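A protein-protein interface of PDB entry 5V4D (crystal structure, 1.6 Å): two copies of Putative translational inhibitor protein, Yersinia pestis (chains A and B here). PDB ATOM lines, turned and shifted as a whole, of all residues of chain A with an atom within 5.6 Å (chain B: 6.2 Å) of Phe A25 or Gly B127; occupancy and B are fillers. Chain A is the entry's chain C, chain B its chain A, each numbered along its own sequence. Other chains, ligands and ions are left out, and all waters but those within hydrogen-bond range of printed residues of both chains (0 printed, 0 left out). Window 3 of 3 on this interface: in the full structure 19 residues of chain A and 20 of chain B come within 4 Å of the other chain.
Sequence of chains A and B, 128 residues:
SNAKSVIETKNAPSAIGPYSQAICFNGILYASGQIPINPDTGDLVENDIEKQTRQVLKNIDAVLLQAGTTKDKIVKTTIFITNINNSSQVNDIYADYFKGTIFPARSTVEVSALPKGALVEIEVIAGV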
ATOM      1  N   ALA A   3       9.169  -9.666 -21.411  1.00  0.00           N
ATOM      2  CA  ALA A   3       8.668  -8.858 -20.305  1.00  0.00           C
ATOM      3  C   ALA A   3       9.388  -7.523 -20.267  1.00  0.00           C
ATOM      4  O   ALA A   3      10.489  -7.353 -20.808  1.00  0.00           O
ATOM      5  CB  ALA A   3       8.833  -9.570 -18.995  1.00  0.00           C
ATOM      6  N   LYS A   4       8.775  -6.570 -19.588  1.00  0.00           N
ATOM      7  CA  LYS A   4       9.403  -5.267 -19.532  1.00  0.00           C
ATOM      8  C   LYS A   4      10.619  -5.319 -18.617  1.00  0.00           C
ATOM      9  O   LYS A   4      10.700  -6.139 -17.703  1.00  0.00           O
ATOM     10  CB  LYS A   4       8.388  -4.212 -19.099  1.00  0.00           C
ATOM     11  CG  LYS A   4       8.191  -4.062 -17.642  1.00  0.00           C
ATOM     12  CD  LYS A   4       6.812  -3.369 -17.358  1.00  0.00           C
ATOM     13  CE  LYS A   4       7.002  -2.314 -16.296  1.00  0.00           C
ATOM     14  NZ  LYS A   4       5.807  -2.041 -15.429  1.00  0.00           N
ATOM     15  N   SER A   5      11.590  -4.434 -18.902  1.00  0.00           N
ATOM     16  CA  SER A   5      12.806  -4.338 -18.110  1.00  0.00           C
ATOM     17  C   SER A   5      13.107  -2.866 -17.861  1.00  0.00           C
ATOM     18  O   SER A   5      12.771  -2.004 -18.681  1.00  0.00           O
ATOM     19  CB  SER A   5      14.007  -5.005 -18.829  1.00  0.00           C
ATOM     20  OG  SER A   5      14.139  -4.454 -20.120  1.00  0.00           O
ATOM     21  N   ILE A  23      11.787   2.241 -19.866  1.00  0.00           N
ATOM     22  CA  ILE A  23      11.353   0.852 -19.833  1.00  0.00           C
ATOM     23  C   ILE A  23      11.583   0.292 -21.226  1.00  0.00           C
ATOM     24  O   ILE A  23      11.244   0.948 -22.214  1.00  0.00           O
ATOM     25  CB  ILE A  23       9.859   0.713 -19.458  1.00  0.00           C
ATOM     26  CG1 ILE A  23       9.585   1.120 -17.996  1.00  0.00           C
ATOM     27  CG2 ILE A  23       9.364  -0.721 -19.682  1.00  0.00           C
ATOM     28  CD1 ILE A  23      10.294   0.292 -16.876  1.00  0.00           C
ATOM     29  N   CYS A  24      12.123  -0.924 -21.309  1.00  0.00           N
ATOM     30  CA  CYS A  24      12.226  -1.631 -22.579  1.00  0.00           C
ATOM     31  C   CYS A  24      11.186  -2.733 -22.639  1.00  0.00           C
ATOM     32  O   CYS A  24      10.974  -3.449 -21.652  1.00  0.00           O
ATOM     33  CB  CYS A  24      13.584  -2.279 -22.771  1.00  0.00           C
ATOM     34  SG  CYS A  24      14.884  -1.088 -22.910  1.00  0.00           S
ATOM     35  N   PHE A  25      10.549  -2.863 -23.794  1.00  0.00           N
ATOM     36  CA  PHE A  25       9.544  -3.911 -23.964  1.00  0.00           C
ATOM     37  C   PHE A  25       9.468  -4.287 -25.435  1.00  0.00           C
ATOM     38  O   PHE A  25       9.334  -3.408 -26.288  1.00  0.00           O
ATOM     39  CB  PHE A  25       8.178  -3.441 -23.439  1.00  0.00           C
ATOM     40  CG  PHE A  25       7.138  -4.506 -23.515  1.00  0.00           C
ATOM     41  CD1 PHE A  25       6.229  -4.528 -24.549  1.00  0.00           C
ATOM     42  CD2 PHE A  25       7.134  -5.511 -22.593  1.00  0.00           C
ATOM     43  CE1 PHE A  25       5.296  -5.546 -24.643  1.00  0.00           C
ATOM     44  CE2 PHE A  25       6.210  -6.556 -22.671  1.00  0.00           C
ATOM     45  CZ  PHE A  25       5.287  -6.559 -23.704  1.00  0.00           C
ATOM     46  N   ASN A  26       9.626  -5.583 -25.709  1.00  0.00           N
ATOM     47  CA  ASN A  26       9.545  -6.126 -27.057  1.00  0.00           C
ATOM     48  C   ASN A  26      10.444  -5.355 -28.021  1.00  0.00           C
ATOM     49  O   ASN A  26      10.061  -5.036 -29.148  1.00  0.00           O
ATOM     50  CB  ASN A  26       8.089  -6.150 -27.526  1.00  0.00           C
ATOM     51  CG  ASN A  26       7.259  -7.201 -26.785  1.00  0.00           C
ATOM     52  OD1 ASN A  26       7.785  -7.965 -25.973  1.00  0.00           O
ATOM     53  ND2 ASN A  26       5.963  -7.234 -27.062  1.00  0.00           N
ATOM     54  N   GLY A  27      11.655  -5.047 -27.566  1.00  0.00           N
ATOM     55  CA  GLY A  27      12.646  -4.442 -28.432  1.00  0.00           C
ATOM     56  C   GLY A  27      12.502  -2.950 -28.654  1.00  0.00           C
ATOM     57  O   GLY A  27      13.217  -2.393 -29.501  1.00  0.00           O
ATOM     58  N   ILE A  28      11.649  -2.281 -27.889  1.00  0.00           N
ATOM     59  CA  ILE A  28      11.443  -0.834 -27.981  1.00  0.00           C
ATOM     60  C   ILE A  28      11.796  -0.217 -26.634  1.00  0.00           C
ATOM     61  O   ILE A  28      11.387  -0.735 -25.593  1.00  0.00           O
ATOM     62  CB  ILE A  28       9.991  -0.498 -28.355  1.00  0.00           C
ATOM     63  CG1 ILE A  28       9.649  -1.094 -29.732  1.00  0.00           C
ATOM     64  CG2 ILE A  28       9.777   0.989 -28.319  1.00  0.00           C
ATOM     65  CD1 ILE A  28      10.469  -0.501 -30.861  1.00  0.00           C
ATOM     66  N   LEU A  29      12.548   0.876 -26.656  1.00  0.00           N
ATOM     67  CA  LEU A  29      12.871   1.649 -25.460  1.00  0.00           C
ATOM     68  C   LEU A  29      11.893   2.810 -25.339  1.00  0.00           C
ATOM     69  O   LEU A  29      11.821   3.653 -26.237  1.00  0.00           O
ATOM     70  CB  LEU A  29      14.308   2.162 -25.540  1.00  0.00           C
ATOM     71  CG  LEU A  29      14.801   3.032 -24.384  1.00  0.00           C
ATOM     72  CD1 LEU A  29      14.964   2.206 -23.176  1.00  0.00           C
ATOM     73  CD2 LEU A  29      16.163   3.579 -24.777  1.00  0.00           C
ATOM     74  N   TYR A  30      11.109   2.830 -24.248  1.00  0.00           N
ATOM     75  CA  TYR A  30      10.216   3.946 -23.951  1.00  0.00           C
ATOM     76  C   TYR A  30      10.907   4.778 -22.892  1.00  0.00           C
ATOM     77  O   TYR A  30      10.963   4.387 -21.715  1.00  0.00           O
ATOM     78  CB  TYR A  30       8.848   3.449 -23.471  1.00  0.00           C
ATOM     79  CG  TYR A  30       8.166   2.607 -24.509  1.00  0.00           C
ATOM     80  CD1 TYR A  30       7.300   3.185 -25.443  1.00  0.00           C
ATOM     81  CD2 TYR A  30       8.417   1.218 -24.593  1.00  0.00           C
ATOM     82  CE1 TYR A  30       6.687   2.409 -26.436  1.00  0.00           C
ATOM     83  CE2 TYR A  30       7.773   0.449 -25.542  1.00  0.00           C
ATOM     84  CZ  TYR A  30       6.925   1.045 -26.463  1.00  0.00           C
ATOM     85  OH  TYR A  30       6.325   0.251 -27.427  1.00  0.00           O
ATOM     86  N   GLY B  27       0.567  -7.079 -29.523  1.00  0.00           N
ATOM     87  CA  GLY B  27       1.060  -7.277 -28.170  1.00  0.00           C
ATOM     88  C   GLY B  27       1.082  -6.037 -27.290  1.00  0.00           C
ATOM     89  O   GLY B  27       1.468  -6.143 -26.114  1.00  0.00           O
ATOM     90  N   ILE B  28       0.633  -4.893 -27.792  1.00  0.00           N
ATOM     91  CA  ILE B  28       0.570  -3.652 -27.026  1.00  0.00           C
ATOM     92  C   ILE B  28      -0.880  -3.218 -26.862  1.00  0.00           C
ATOM     93  O   ILE B  28      -1.639  -3.204 -27.839  1.00  0.00           O
ATOM     94  CB  ILE B  28       1.352  -2.514 -27.706  1.00  0.00           C
ATOM     95  CG1 ILE B  28       2.827  -2.898 -27.888  1.00  0.00           C
ATOM     96  CG2 ILE B  28       1.144  -1.201 -26.926  1.00  0.00           C
ATOM     97  CD1 ILE B  28       3.575  -2.923 -26.597  1.00  0.00           C
ATOM     98  N   LEU B  29      -1.260  -2.855 -25.630  1.00  0.00           N
ATOM     99  CA  LEU B  29      -2.543  -2.231 -25.349  1.00  0.00           C
ATOM    100  C   LEU B  29      -2.376  -0.714 -25.338  1.00  0.00           C
ATOM    101  O   LEU B  29      -1.620  -0.173 -24.519  1.00  0.00           O
ATOM    102  CB  LEU B  29      -3.066  -2.700 -23.993  1.00  0.00           C
ATOM    103  CG  LEU B  29      -4.352  -2.054 -23.508  1.00  0.00           C
ATOM    104  CD1 LEU B  29      -5.405  -2.339 -24.496  1.00  0.00           C
ATOM    105  CD2 LEU B  29      -4.761  -2.634 -22.161  1.00  0.00           C
ATOM    106  N   THR B  69      -5.092  -8.006 -18.783  1.00  0.00           N
ATOM    107  CA  THR B  69      -3.735  -7.683 -18.347  1.00  0.00           C
ATOM    108  C   THR B  69      -3.832  -6.927 -17.021  1.00  0.00           C
ATOM    109  O   THR B  69      -4.918  -6.897 -16.419  1.00  0.00           O
ATOM    110  CB  THR B  69      -2.982  -6.907 -19.435  1.00  0.00           C
ATOM    111  OG1 THR B  69      -1.590  -6.829 -19.066  1.00  0.00           O
ATOM    112  CG2 THR B  69      -3.513  -5.494 -19.612  1.00  0.00           C
ATOM    113  N   THR B  70      -2.714  -6.382 -16.519  1.00  0.00           N
ATOM    114  CA  THR B  70      -2.715  -5.747 -15.203  1.00  0.00           C
ATOM    115  C   THR B  70      -1.772  -4.560 -15.229  1.00  0.00           C
ATOM    116  O   THR B  70      -0.985  -4.390 -16.161  1.00  0.00           O
ATOM    117  CB  THR B  70      -2.258  -6.666 -14.074  1.00  0.00           C
ATOM    118  OG1 THR B  70      -0.907  -7.046 -14.315  1.00  0.00           O
ATOM    119  CG2 THR B  70      -3.136  -7.929 -13.923  1.00  0.00           C
ATOM    120  N   LYS B  73       1.995  -4.554 -16.105  1.00  0.00           N
ATOM    121  CA  LYS B  73       2.439  -4.584 -17.497  1.00  0.00           C
ATOM    122  C   LYS B  73       2.481  -3.210 -18.165  1.00  0.00           C
ATOM    123  O   LYS B  73       2.872  -3.132 -19.341  1.00  0.00           O
ATOM    124  CB  LYS B  73       1.520  -5.482 -18.337  1.00  0.00           C
ATOM    125  CG  LYS B  73       1.487  -6.934 -17.873  1.00  0.00           C
ATOM    126  CD  LYS B  73       2.872  -7.482 -17.774  1.00  0.00           C
ATOM    127  CE  LYS B  73       2.815  -8.948 -17.351  1.00  0.00           C
ATOM    128  NZ  LYS B  73       2.066  -9.757 -18.364  1.00  0.00           N
ATOM    129  N   ILE B  74       2.136  -2.131 -17.456  1.00  0.00           N
ATOM    130  CA  ILE B  74       2.180  -0.801 -18.060  1.00  0.00           C
ATOM    131  C   ILE B  74       3.629  -0.416 -18.281  1.00  0.00           C
ATOM    132  O   ILE B  74       4.468  -0.552 -17.386  1.00  0.00           O
ATOM    133  CB  ILE B  74       1.428   0.223 -17.199  1.00  0.00           C
ATOM    134  CG1 ILE B  74      -0.075  -0.102 -17.286  1.00  0.00           C
ATOM    135  CG2 ILE B  74       1.685   1.687 -17.726  1.00  0.00           C
ATOM    136  CD1 ILE B  74      -0.963   0.780 -16.335  1.00  0.00           C
ATOM    137  N   VAL B  75       3.921   0.036 -19.497  1.00  0.00           N
ATOM    138  CA  VAL B  75       5.263   0.351 -19.933  1.00  0.00           C
ATOM    139  C   VAL B  75       5.545   1.844 -19.834  1.00  0.00           C
ATOM    140  O   VAL B  75       6.641   2.250 -19.450  1.00  0.00           O
ATOM    141  CB  VAL B  75       5.409  -0.171 -21.383  1.00  0.00           C
ATOM    142  CG1 VAL B  75       6.569   0.400 -22.048  1.00  0.00           C
ATOM    143  CG2 VAL B  75       5.532  -1.715 -21.360  1.00  0.00           C
ATOM    144  N   ILE B 125       0.190   2.916 -22.021  1.00  0.00           N
ATOM    145  CA  ILE B 125       0.340   1.754 -22.886  1.00  0.00           C
ATOM    146  C   ILE B 125       0.842   0.610 -22.028  1.00  0.00           C
ATOM    147  O   ILE B 125       1.582   0.805 -21.058  1.00  0.00           O
ATOM    148  CB  ILE B 125       1.270   1.954 -24.097  1.00  0.00           C
ATOM    149  CG1 ILE B 125       2.668   2.363 -23.645  1.00  0.00           C
ATOM    150  CG2 ILE B 125       0.635   2.931 -25.095  1.00  0.00           C
ATOM    151  CD1 ILE B 125       3.729   2.104 -24.724  1.00  0.00           C
ATOM    152  N   ALA B 126       0.411  -0.597 -22.380  1.00  0.00           N
ATOM    153  CA  ALA B 126       0.746  -1.770 -21.594  1.00  0.00           C
ATOM    154  C   ALA B 126       1.126  -2.919 -22.506  1.00  0.00           C
ATOM    155  O   ALA B 126       0.666  -3.014 -23.636  1.00  0.00           O
ATOM    156  CB  ALA B 126      -0.412  -2.222 -20.699  1.00  0.00           C
ATOM    157  N   GLY B 127       1.816  -3.908 -21.948  1.00  0.00           N
ATOM    158  CA  GLY B 127       1.836  -5.217 -22.583  1.00  0.00           C
ATOM    159  C   GLY B 127       0.527  -5.962 -22.381  1.00  0.00           C
ATOM    160  O   GLY B 127      -0.135  -5.834 -21.353  1.00  0.00           O
ATOM    161  N   VAL B 128       0.143  -6.750 -23.384  1.00  0.00           N
ATOM    162  CA  VAL B 128      -1.074  -7.544 -23.276  1.00  0.00           C
ATOM    163  C   VAL B 128      -0.830  -8.746 -22.382  1.00  0.00           C
ATOM    164  O   VAL B 128      -1.755  -9.499 -22.086  1.00  0.00           O
ATOM    165  CB  VAL B 128      -1.591  -8.007 -24.647  1.00  0.00           C
ATOM    166  CG1 VAL B 128      -2.053  -6.813 -25.475  1.00  0.00           C
ATOM    167  CG2 VAL B 128      -0.529  -8.810 -25.360  1.00  0.00           C
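Printed residues of chain A that touch a printed residue of chain B: Lys A4, Ile A23, Phe A25 and Tyr A30.
Along chain A the printed residues that touch a printed residue of chain B span positions 4 to 30.
Among the printed residues, 7 pairs touch across the chains.
Among the printed residues, pairs that only touch across the chains: Ile A23 with Val B75, Phe A25 with Ile B28, Phe A25 with Val B75, Phe A25 with Gly B127, Tyr A30 with Val B75 and Tyr A30 with Ile B125.
The side-chain hydroxyl (OG1) of Thr B69 sits at hydrogen-bond distance from the backbone carbonyl oxygen (O) of Gly B127 (2.9 Å).
O of Lys B73 sits at hydrogen-bond distance from N of Gly B127 (2.9 Å).
The backbone NH (N) of Val B75 lies within hydrogen-bond range of the backbone carbonyl oxygen (O) of Ile B125, at 2.9 Å.
O of Ile A23 is in hydrogen-bond range of N of Tyr A30 (2.8 Å).
O of Ile B74 is in hydrogen-bond range of NZ of Lys A4 (2.8 Å).
3 positions are printed for both chains.
Of the 7 pairs that touch across the chains among the printed residues, none has its exchanged pair printed and touching as well.
Of the printed residues of chain B, Lys A4 touches Ile B74.
Of the printed residues of chain B, Ile A23 touches Val B75.
Printed residues of chain B within 4 Å of Phe A25: Ile B28, Val B75 and Gly B127.
Printed residues of chain B within 4 Å of Tyr A30: Val B75 and Ile B125.
Printed residues of chain A within 4 Å of Ile B74: Lys A4 (2.8 Å).
Of the printed residues of chain A, Val B75 touches Ile A23, Phe A25 and Tyr A30.
The nearest printed residue of chain B that does not touch Phe A25 is Gly B27 (4.1 Å).
The nearest printed residue of chain A that does not touch Gly B127 is Asn A26 (6.4 Å).
The nearest printed residue of chain A that does not touch Val B75 is Lys A4 (4.4 Å).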
